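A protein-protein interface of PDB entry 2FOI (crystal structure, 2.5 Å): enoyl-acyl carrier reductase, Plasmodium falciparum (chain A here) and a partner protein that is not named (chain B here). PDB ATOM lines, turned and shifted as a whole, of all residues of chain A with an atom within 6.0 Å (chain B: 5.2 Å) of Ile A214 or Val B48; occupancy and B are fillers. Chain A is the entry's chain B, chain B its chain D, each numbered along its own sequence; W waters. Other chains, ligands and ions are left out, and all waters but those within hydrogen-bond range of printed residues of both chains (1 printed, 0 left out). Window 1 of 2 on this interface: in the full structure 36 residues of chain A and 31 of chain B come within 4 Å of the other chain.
The backbone carbonyl oxygen of Thr A213 is in hydrogen-bond range of the backbone NH of Ile B46 (2.8 Å).
The backbone NH (N) of Gly A217 sits at hydrogen-bond distance from the backbone carbonyl oxygen (O) of Val B48 (3.0 Å).
The backbone NH (N) of Ser A215 lies within hydrogen-bond range of the backbone carbonyl oxygen (O) of Ile B46 (2.9 Å).
The backbone NH of Val B48 sits at hydrogen-bond distance from the backbone carbonyl oxygen of Ser A215, 2.9 Å away.
The backbone carbonyl oxygen (O) of Ile A214 is in hydrogen-bond range of the backbone NH (N) of Thr A170, at 2.6 Å.
O of Ser A168 is in hydrogen-bond range of N of Ile A214 (2.9 Å).
The backbone carbonyl oxygen (O) of Thr A170 sits at hydrogen-bond distance from the backbone NH (N) of Ala A216, at 3.1 Å.
The side-chain hydroxyl (OG) of Ser A168 lies within hydrogen-bond range of the side-chain hydroxyl (OG1) of Thr A213 (2.9 Å).
The side-chain hydroxyl (OH) of Tyr A15 is in hydrogen-bond range of the backbone carbonyl oxygen (O) of Gly A217, 2.7 Å away.
Among the printed residues, pairs that only touch across the chains: Tyr A15 with Ile B26 (3.1 Å), Ser A215 with Tyr B47 (3.2 Å), Ile A214 with Ile B46 (3.2 Å), Ala A216 with Val B48 (3.3 Å), Gly A217 with Leu B21 (3.4 Å), Tyr A15 with Leu B21 (3.5 Å), Ile A167 with Ala B30 (3.5 Å), Gly A217 with Asp B49 (3.5 Å), Ile A214 with Val B48 (3.7 Å), Ile A214 with Ala B30 (3.7 Å), Ile A214 with Leu B33 (3.7 Å), Ala A216 with Ile B26 (3.8 Å), Ile A167 with Leu B33 (3.9 Å) and Leu A169 with Ile B26 (3.9 Å).
Ile A214 touches just these residues of chain B: Ala B30, Leu B33, Ile B46 and Val B48.
Printed residues of chain A within 4 Å of Ala B30: Ile A167 and Ile A214.
Val B48 touches just these residues of chain A: Ile A214, Ser A215, Ala A216 and Gly A217.
Of the printed residues of chain A, Asp B49 touches Gly A217 (3.5 Å).
The nearest residue of chain A that does not touch Val B48 is Tyr A15 (5.3 Å).
Along chain A the printed residues that touch a printed residue of chain B span positions 15 to 217.
Water W1 lies within hydrogen-bond range of the side-chain hydroxyl (OG) of Ser A215 (2.4 Å) and the side-chain hydroxyl (OH) of Tyr B47 (2.8 Å).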
ATOM      1  N   TYR A  15      23.868 -32.961 -17.217  1.00  0.00           N
ATOM      2  CA  TYR A  15      22.785 -32.097 -17.708  1.00  0.00           C
ATOM      3  C   TYR A  15      23.272 -31.173 -18.818  1.00  0.00           C
ATOM      4  O   TYR A  15      22.506 -30.829 -19.724  1.00  0.00           O
ATOM      5  CB  TYR A  15      22.160 -31.282 -16.574  1.00  0.00           C
ATOM      6  CG  TYR A  15      21.162 -32.037 -15.693  1.00  0.00           C
ATOM      7  CD1 TYR A  15      19.992 -32.541 -16.220  1.00  0.00           C
ATOM      8  CD2 TYR A  15      21.380 -32.190 -14.329  1.00  0.00           C
ATOM      9  CE1 TYR A  15      19.072 -33.210 -15.429  1.00  0.00           C
ATOM     10  CE2 TYR A  15      20.462 -32.849 -13.531  1.00  0.00           C
ATOM     11  CZ  TYR A  15      19.307 -33.357 -14.104  1.00  0.00           C
ATOM     12  OH  TYR A  15      18.391 -34.019 -13.339  1.00  0.00           O
ATOM     13  N   ILE A 167      21.258 -19.202 -17.873  1.00  0.00           N
ATOM     14  CA  ILE A 167      20.749 -20.108 -16.843  1.00  0.00           C
ATOM     15  C   ILE A 167      21.848 -20.888 -16.129  1.00  0.00           C
ATOM     16  O   ILE A 167      22.911 -21.146 -16.700  1.00  0.00           O
ATOM     17  CB  ILE A 167      19.765 -21.141 -17.385  1.00  0.00           C
ATOM     18  CG1 ILE A 167      20.500 -22.114 -18.289  1.00  0.00           C
ATOM     19  CG2 ILE A 167      18.562 -20.486 -18.055  1.00  0.00           C
ATOM     20  CD1 ILE A 167      19.840 -23.460 -18.334  1.00  0.00           C
ATOM     21  N   SER A 168      21.569 -21.276 -14.886  1.00  0.00           N
ATOM     22  CA  SER A 168      22.452 -22.152 -14.118  1.00  0.00           C
ATOM     23  C   SER A 168      21.605 -23.303 -13.600  1.00  0.00           C
ATOM     24  O   SER A 168      20.379 -23.270 -13.775  1.00  0.00           O
ATOM     25  CB  SER A 168      23.088 -21.405 -12.951  1.00  0.00           C
ATOM     26  OG  SER A 168      22.137 -21.179 -11.914  1.00  0.00           O
ATOM     27  N   LEU A 169      22.249 -24.317 -12.999  1.00  0.00           N
ATOM     28  CA  LEU A 169      21.535 -25.447 -12.376  1.00  0.00           C
ATOM     29  C   LEU A 169      21.654 -25.394 -10.863  1.00  0.00           C
ATOM     30  O   LEU A 169      22.735 -25.136 -10.314  1.00  0.00           O
ATOM     31  CB  LEU A 169      22.081 -26.790 -12.832  1.00  0.00           C
ATOM     32  CG  LEU A 169      21.962 -27.379 -14.251  1.00  0.00           C
ATOM     33  CD1 LEU A 169      20.548 -27.751 -14.640  1.00  0.00           C
ATOM     34  CD2 LEU A 169      22.532 -26.455 -15.283  1.00  0.00           C
ATOM     35  N   THR A 170      20.552 -25.640 -10.168  1.00  0.00           N
ATOM     36  CA  THR A 170      20.659 -25.770  -8.714  1.00  0.00           C
ATOM     37  C   THR A 170      20.035 -27.064  -8.179  1.00  0.00           C
ATOM     38  O   THR A 170      19.540 -27.894  -8.947  1.00  0.00           O
ATOM     39  CB  THR A 170      20.082 -24.543  -7.983  1.00  0.00           C
ATOM     40  OG1 THR A 170      20.232 -24.733  -6.571  1.00  0.00           O
ATOM     41  CG2 THR A 170      18.610 -24.338  -8.347  1.00  0.00           C
ATOM     42  N   TYR A 171      20.046 -27.226  -6.862  1.00  0.00           N
ATOM     43  CA  TYR A 171      19.458 -28.394  -6.241  1.00  0.00           C
ATOM     44  C   TYR A 171      18.728 -28.043  -4.923  1.00  0.00           C
ATOM     45  O   TYR A 171      19.145 -27.169  -4.161  1.00  0.00           O
ATOM     46  CB  TYR A 171      20.506 -29.506  -6.087  1.00  0.00           C
ATOM     47  CG  TYR A 171      19.958 -30.777  -5.481  1.00  0.00           C
ATOM     48  CD1 TYR A 171      18.995 -31.534  -6.129  1.00  0.00           C
ATOM     49  CD2 TYR A 171      20.404 -31.211  -4.255  1.00  0.00           C
ATOM     50  CE1 TYR A 171      18.489 -32.683  -5.550  1.00  0.00           C
ATOM     51  CE2 TYR A 171      19.919 -32.360  -3.679  1.00  0.00           C
ATOM     52  CZ  TYR A 171      18.960 -33.082  -4.312  1.00  0.00           C
ATOM     53  OH  TYR A 171      18.481 -34.214  -3.669  1.00  0.00           O
ATOM     54  N   ASN A 212      17.937 -17.068 -14.886  1.00  0.00           N
ATOM     55  CA  ASN A 212      17.139 -17.943 -14.059  1.00  0.00           C
ATOM     56  C   ASN A 212      17.962 -19.155 -13.652  1.00  0.00           C
ATOM     57  O   ASN A 212      19.077 -19.361 -14.145  1.00  0.00           O
ATOM     58  CB  ASN A 212      15.898 -18.378 -14.819  1.00  0.00           C
ATOM     59  CG  ASN A 212      14.967 -17.226 -15.094  1.00  0.00           C
ATOM     60  OD1 ASN A 212      14.230 -16.783 -14.205  1.00  0.00           O
ATOM     61  ND2 ASN A 212      15.000 -16.715 -16.325  1.00  0.00           N
ATOM     62  N   THR A 213      17.437 -19.934 -12.717  1.00  0.00           N
ATOM     63  CA  THR A 213      18.123 -21.151 -12.320  1.00  0.00           C
ATOM     64  C   THR A 213      17.144 -22.327 -12.337  1.00  0.00           C
ATOM     65  O   THR A 213      15.947 -22.171 -12.017  1.00  0.00           O
ATOM     66  CB  THR A 213      18.858 -20.989 -10.969  1.00  0.00           C
ATOM     67  OG1 THR A 213      19.650 -22.151 -10.694  1.00  0.00           O
ATOM     68  CG2 THR A 213      17.902 -20.727  -9.815  1.00  0.00           C
ATOM     69  N   ILE A 214      17.634 -23.482 -12.788  1.00  0.00           N
ATOM     70  CA  ILE A 214      16.826 -24.690 -12.807  1.00  0.00           C
ATOM     71  C   ILE A 214      17.234 -25.599 -11.664  1.00  0.00           C
ATOM     72  O   ILE A 214      18.395 -25.968 -11.558  1.00  0.00           O
ATOM     73  CB  ILE A 214      17.005 -25.458 -14.112  1.00  0.00           C
ATOM     74  CG1 ILE A 214      16.515 -24.635 -15.303  1.00  0.00           C
ATOM     75  CG2 ILE A 214      16.263 -26.790 -14.049  1.00  0.00           C
ATOM     76  CD1 ILE A 214      16.610 -25.369 -16.611  1.00  0.00           C
ATOM     77  N   SER A 215      16.281 -25.929 -10.794  1.00  0.00           N
ATOM     78  CA  SER A 215      16.503 -26.868  -9.716  1.00  0.00           C
ATOM     79  C   SER A 215      16.109 -28.268 -10.207  1.00  0.00           C
ATOM     80  O   SER A 215      14.932 -28.635 -10.263  1.00  0.00           O
ATOM     81  CB  SER A 215      15.696 -26.467  -8.480  1.00  0.00           C
ATOM     82  OG  SER A 215      16.174 -27.117  -7.312  1.00  0.00           O
ATOM     83  N   ALA A 216      17.113 -29.048 -10.576  1.00  0.00           N
ATOM     84  CA  ALA A 216      16.888 -30.350 -11.215  1.00  0.00           C
ATOM     85  C   ALA A 216      16.733 -31.464 -10.204  1.00  0.00           C
ATOM     86  O   ALA A 216      17.226 -31.376  -9.076  1.00  0.00           O
ATOM     87  CB  ALA A 216      18.038 -30.655 -12.133  1.00  0.00           C
ATOM     88  N   GLY A 217      16.030 -32.511 -10.604  1.00  0.00           N
ATOM     89  CA  GLY A 217      15.947 -33.724  -9.801  1.00  0.00           C
ATOM     90  C   GLY A 217      17.244 -34.504  -9.982  1.00  0.00           C
ATOM     91  O   GLY A 217      18.159 -34.052 -10.694  1.00  0.00           O
ATOM     92  N   LEU B  21      13.666 -39.531 -14.781  1.00  0.00           N
ATOM     93  CA  LEU B  21      13.985 -38.117 -15.070  1.00  0.00           C
ATOM     94  C   LEU B  21      15.195 -38.078 -15.951  1.00  0.00           C
ATOM     95  O   LEU B  21      16.219 -38.643 -15.602  1.00  0.00           O
ATOM     96  CB  LEU B  21      14.247 -37.307 -13.798  1.00  0.00           C
ATOM     97  CG  LEU B  21      14.629 -35.841 -14.062  1.00  0.00           C
ATOM     98  CD1 LEU B  21      13.411 -35.051 -14.616  1.00  0.00           C
ATOM     99  CD2 LEU B  21      15.184 -35.199 -12.812  1.00  0.00           C
ATOM    100  N   ASP B  25      15.114 -33.817 -20.229  1.00  0.00           N
ATOM    101  CA  ASP B  25      13.954 -33.163 -19.622  1.00  0.00           C
ATOM    102  C   ASP B  25      14.351 -31.802 -19.062  1.00  0.00           C
ATOM    103  O   ASP B  25      13.596 -30.844 -19.147  1.00  0.00           O
ATOM    104  CB  ASP B  25      13.332 -34.020 -18.525  1.00  0.00           C
ATOM    105  CG  ASP B  25      12.669 -35.266 -19.077  1.00  0.00           C
ATOM    106  OD1 ASP B  25      12.260 -35.253 -20.265  1.00  0.00           O
ATOM    107  OD2 ASP B  25      12.550 -36.257 -18.328  1.00  0.00           O
ATOM    108  N   ILE B  26      15.544 -31.699 -18.497  1.00  0.00           N
ATOM    109  CA  ILE B  26      15.994 -30.402 -18.050  1.00  0.00           C
ATOM    110  C   ILE B  26      16.355 -29.606 -19.297  1.00  0.00           C
ATOM    111  O   ILE B  26      16.063 -28.395 -19.404  1.00  0.00           O
ATOM    112  CB  ILE B  26      17.211 -30.517 -17.139  1.00  0.00           C
ATOM    113  CG1 ILE B  26      16.776 -30.773 -15.686  1.00  0.00           C
ATOM    114  CG2 ILE B  26      18.087 -29.263 -17.261  1.00  0.00           C
ATOM    115  CD1 ILE B  26      16.125 -32.132 -15.461  1.00  0.00           C
ATOM    116  N   VAL B  29      13.723 -27.560 -20.854  1.00  0.00           N
ATOM    117  CA  VAL B  29      13.299 -26.434 -20.027  1.00  0.00           C
ATOM    118  C   VAL B  29      14.378 -25.372 -20.153  1.00  0.00           C
ATOM    119  O   VAL B  29      14.087 -24.182 -20.295  1.00  0.00           O
ATOM    120  CB  VAL B  29      13.144 -26.852 -18.571  1.00  0.00           C
ATOM    121  CG1 VAL B  29      12.684 -25.675 -17.725  1.00  0.00           C
ATOM    122  CG2 VAL B  29      12.173 -27.997 -18.457  1.00  0.00           C
ATOM    123  N   ALA B  30      15.636 -25.810 -20.149  1.00  0.00           N
ATOM    124  CA  ALA B  30      16.743 -24.878 -20.325  1.00  0.00           C
ATOM    125  C   ALA B  30      16.537 -24.129 -21.622  1.00  0.00           C
ATOM    126  O   ALA B  30      16.695 -22.919 -21.696  1.00  0.00           O
ATOM    127  CB  ALA B  30      18.053 -25.627 -20.366  1.00  0.00           C
ATOM    128  N   LEU B  33      13.774 -21.471 -21.371  1.00  0.00           N
ATOM    129  CA  LEU B  33      14.265 -20.326 -20.601  1.00  0.00           C
ATOM    130  C   LEU B  33      15.232 -19.462 -21.396  1.00  0.00           C
ATOM    131  O   LEU B  33      15.227 -18.234 -21.289  1.00  0.00           O
ATOM    132  CB  LEU B  33      14.944 -20.812 -19.333  1.00  0.00           C
ATOM    133  CG  LEU B  33      13.939 -21.319 -18.313  1.00  0.00           C
ATOM    134  CD1 LEU B  33      14.651 -21.967 -17.113  1.00  0.00           C
ATOM    135  CD2 LEU B  33      13.066 -20.140 -17.866  1.00  0.00           C
ATOM    136  N   ILE B  46      13.313 -22.346 -11.184  1.00  0.00           N
ATOM    137  CA  ILE B  46      12.307 -23.202 -11.799  1.00  0.00           C
ATOM    138  C   ILE B  46      12.653 -24.671 -11.572  1.00  0.00           C
ATOM    139  O   ILE B  46      13.725 -25.127 -11.981  1.00  0.00           O
ATOM    140  CB  ILE B  46      12.385 -23.007 -13.293  1.00  0.00           C
ATOM    141  CG1 ILE B  46      12.263 -21.520 -13.597  1.00  0.00           C
ATOM    142  CG2 ILE B  46      11.359 -23.892 -14.013  1.00  0.00           C
ATOM    143  CD1 ILE B  46      10.919 -20.967 -13.236  1.00  0.00           C
ATOM    144  N   TYR B  47      11.735 -25.403 -10.947  1.00  0.00           N
ATOM    145  CA  TYR B  47      11.957 -26.779 -10.523  1.00  0.00           C
ATOM    146  C   TYR B  47      11.599 -27.737 -11.617  1.00  0.00           C
ATOM    147  O   TYR B  47      10.482 -27.720 -12.129  1.00  0.00           O
ATOM    148  CB  TYR B  47      11.084 -27.105  -9.305  1.00  0.00           C
ATOM    149  CG  TYR B  47      11.743 -26.741  -8.006  1.00  0.00           C
ATOM    150  CD1 TYR B  47      12.551 -27.669  -7.317  1.00  0.00           C
ATOM    151  CD2 TYR B  47      11.605 -25.458  -7.479  1.00  0.00           C
ATOM    152  CE1 TYR B  47      13.185 -27.318  -6.123  1.00  0.00           C
ATOM    153  CE2 TYR B  47      12.221 -25.094  -6.279  1.00  0.00           C
ATOM    154  CZ  TYR B  47      13.023 -26.031  -5.616  1.00  0.00           C
ATOM    155  OH  TYR B  47      13.640 -25.687  -4.444  1.00  0.00           O
ATOM    156  N   VAL B  48      12.540 -28.591 -11.980  1.00  0.00           N
ATOM    157  CA  VAL B  48      12.308 -29.575 -13.031  1.00  0.00           C
ATOM    158  C   VAL B  48      12.752 -30.901 -12.418  1.00  0.00           C
ATOM    159  O   VAL B  48      13.943 -31.241 -12.424  1.00  0.00           O
ATOM    160  CB  VAL B  48      13.136 -29.230 -14.298  1.00  0.00           C
ATOM    161  CG1 VAL B  48      12.872 -30.210 -15.422  1.00  0.00           C
ATOM    162  CG2 VAL B  48      12.827 -27.817 -14.748  1.00  0.00           C
ATOM    163  N   ASP B  49      11.801 -31.635 -11.853  1.00  0.00           N
ATOM    164  CA  ASP B  49      12.159 -32.741 -10.982  1.00  0.00           C
ATOM    165  C   ASP B  49      10.952 -33.652 -10.759  1.00  0.00           C
ATOM    166  O   ASP B  49      10.809 -34.243  -9.697  1.00  0.00           O
ATOM    167  CB  ASP B  49      12.641 -32.158  -9.632  1.00  0.00           C
ATOM    168  CG  ASP B  49      11.515 -31.488  -8.862  1.00  0.00           C
ATOM    169  OD1 ASP B  49      10.474 -31.181  -9.503  1.00  0.00           O
ATOM    170  OD2 ASP B  49      11.639 -31.316  -7.628  1.00  0.00           O
ATOM    171  N   ASN B  50      10.054 -33.721 -11.736  1.00  0.00           N
ATOM    172  CA  ASN B  50       8.822 -34.516 -11.613  1.00  0.00           C
ATOM    173  C   ASN B  50       8.032 -34.172 -10.356  1.00  0.00           C
ATOM    174  O   ASN B  50       7.288 -35.003  -9.839  1.00  0.00           O
ATOM    175  CB  ASN B  50       9.115 -36.038 -11.687  1.00  0.00           C
ATOM    176  CG  ASN B  50       9.793 -36.451 -12.998  1.00  0.00           C
ATOM    177  OD1 ASN B  50       9.521 -35.893 -14.065  1.00  0.00           O
ATOM    178  ND2 ASN B  50      10.694 -37.408 -12.915  1.00  0.00           N
HETATM  179  O   HOH W   1      16.236 -25.505  -5.492  1.00  0.00           O
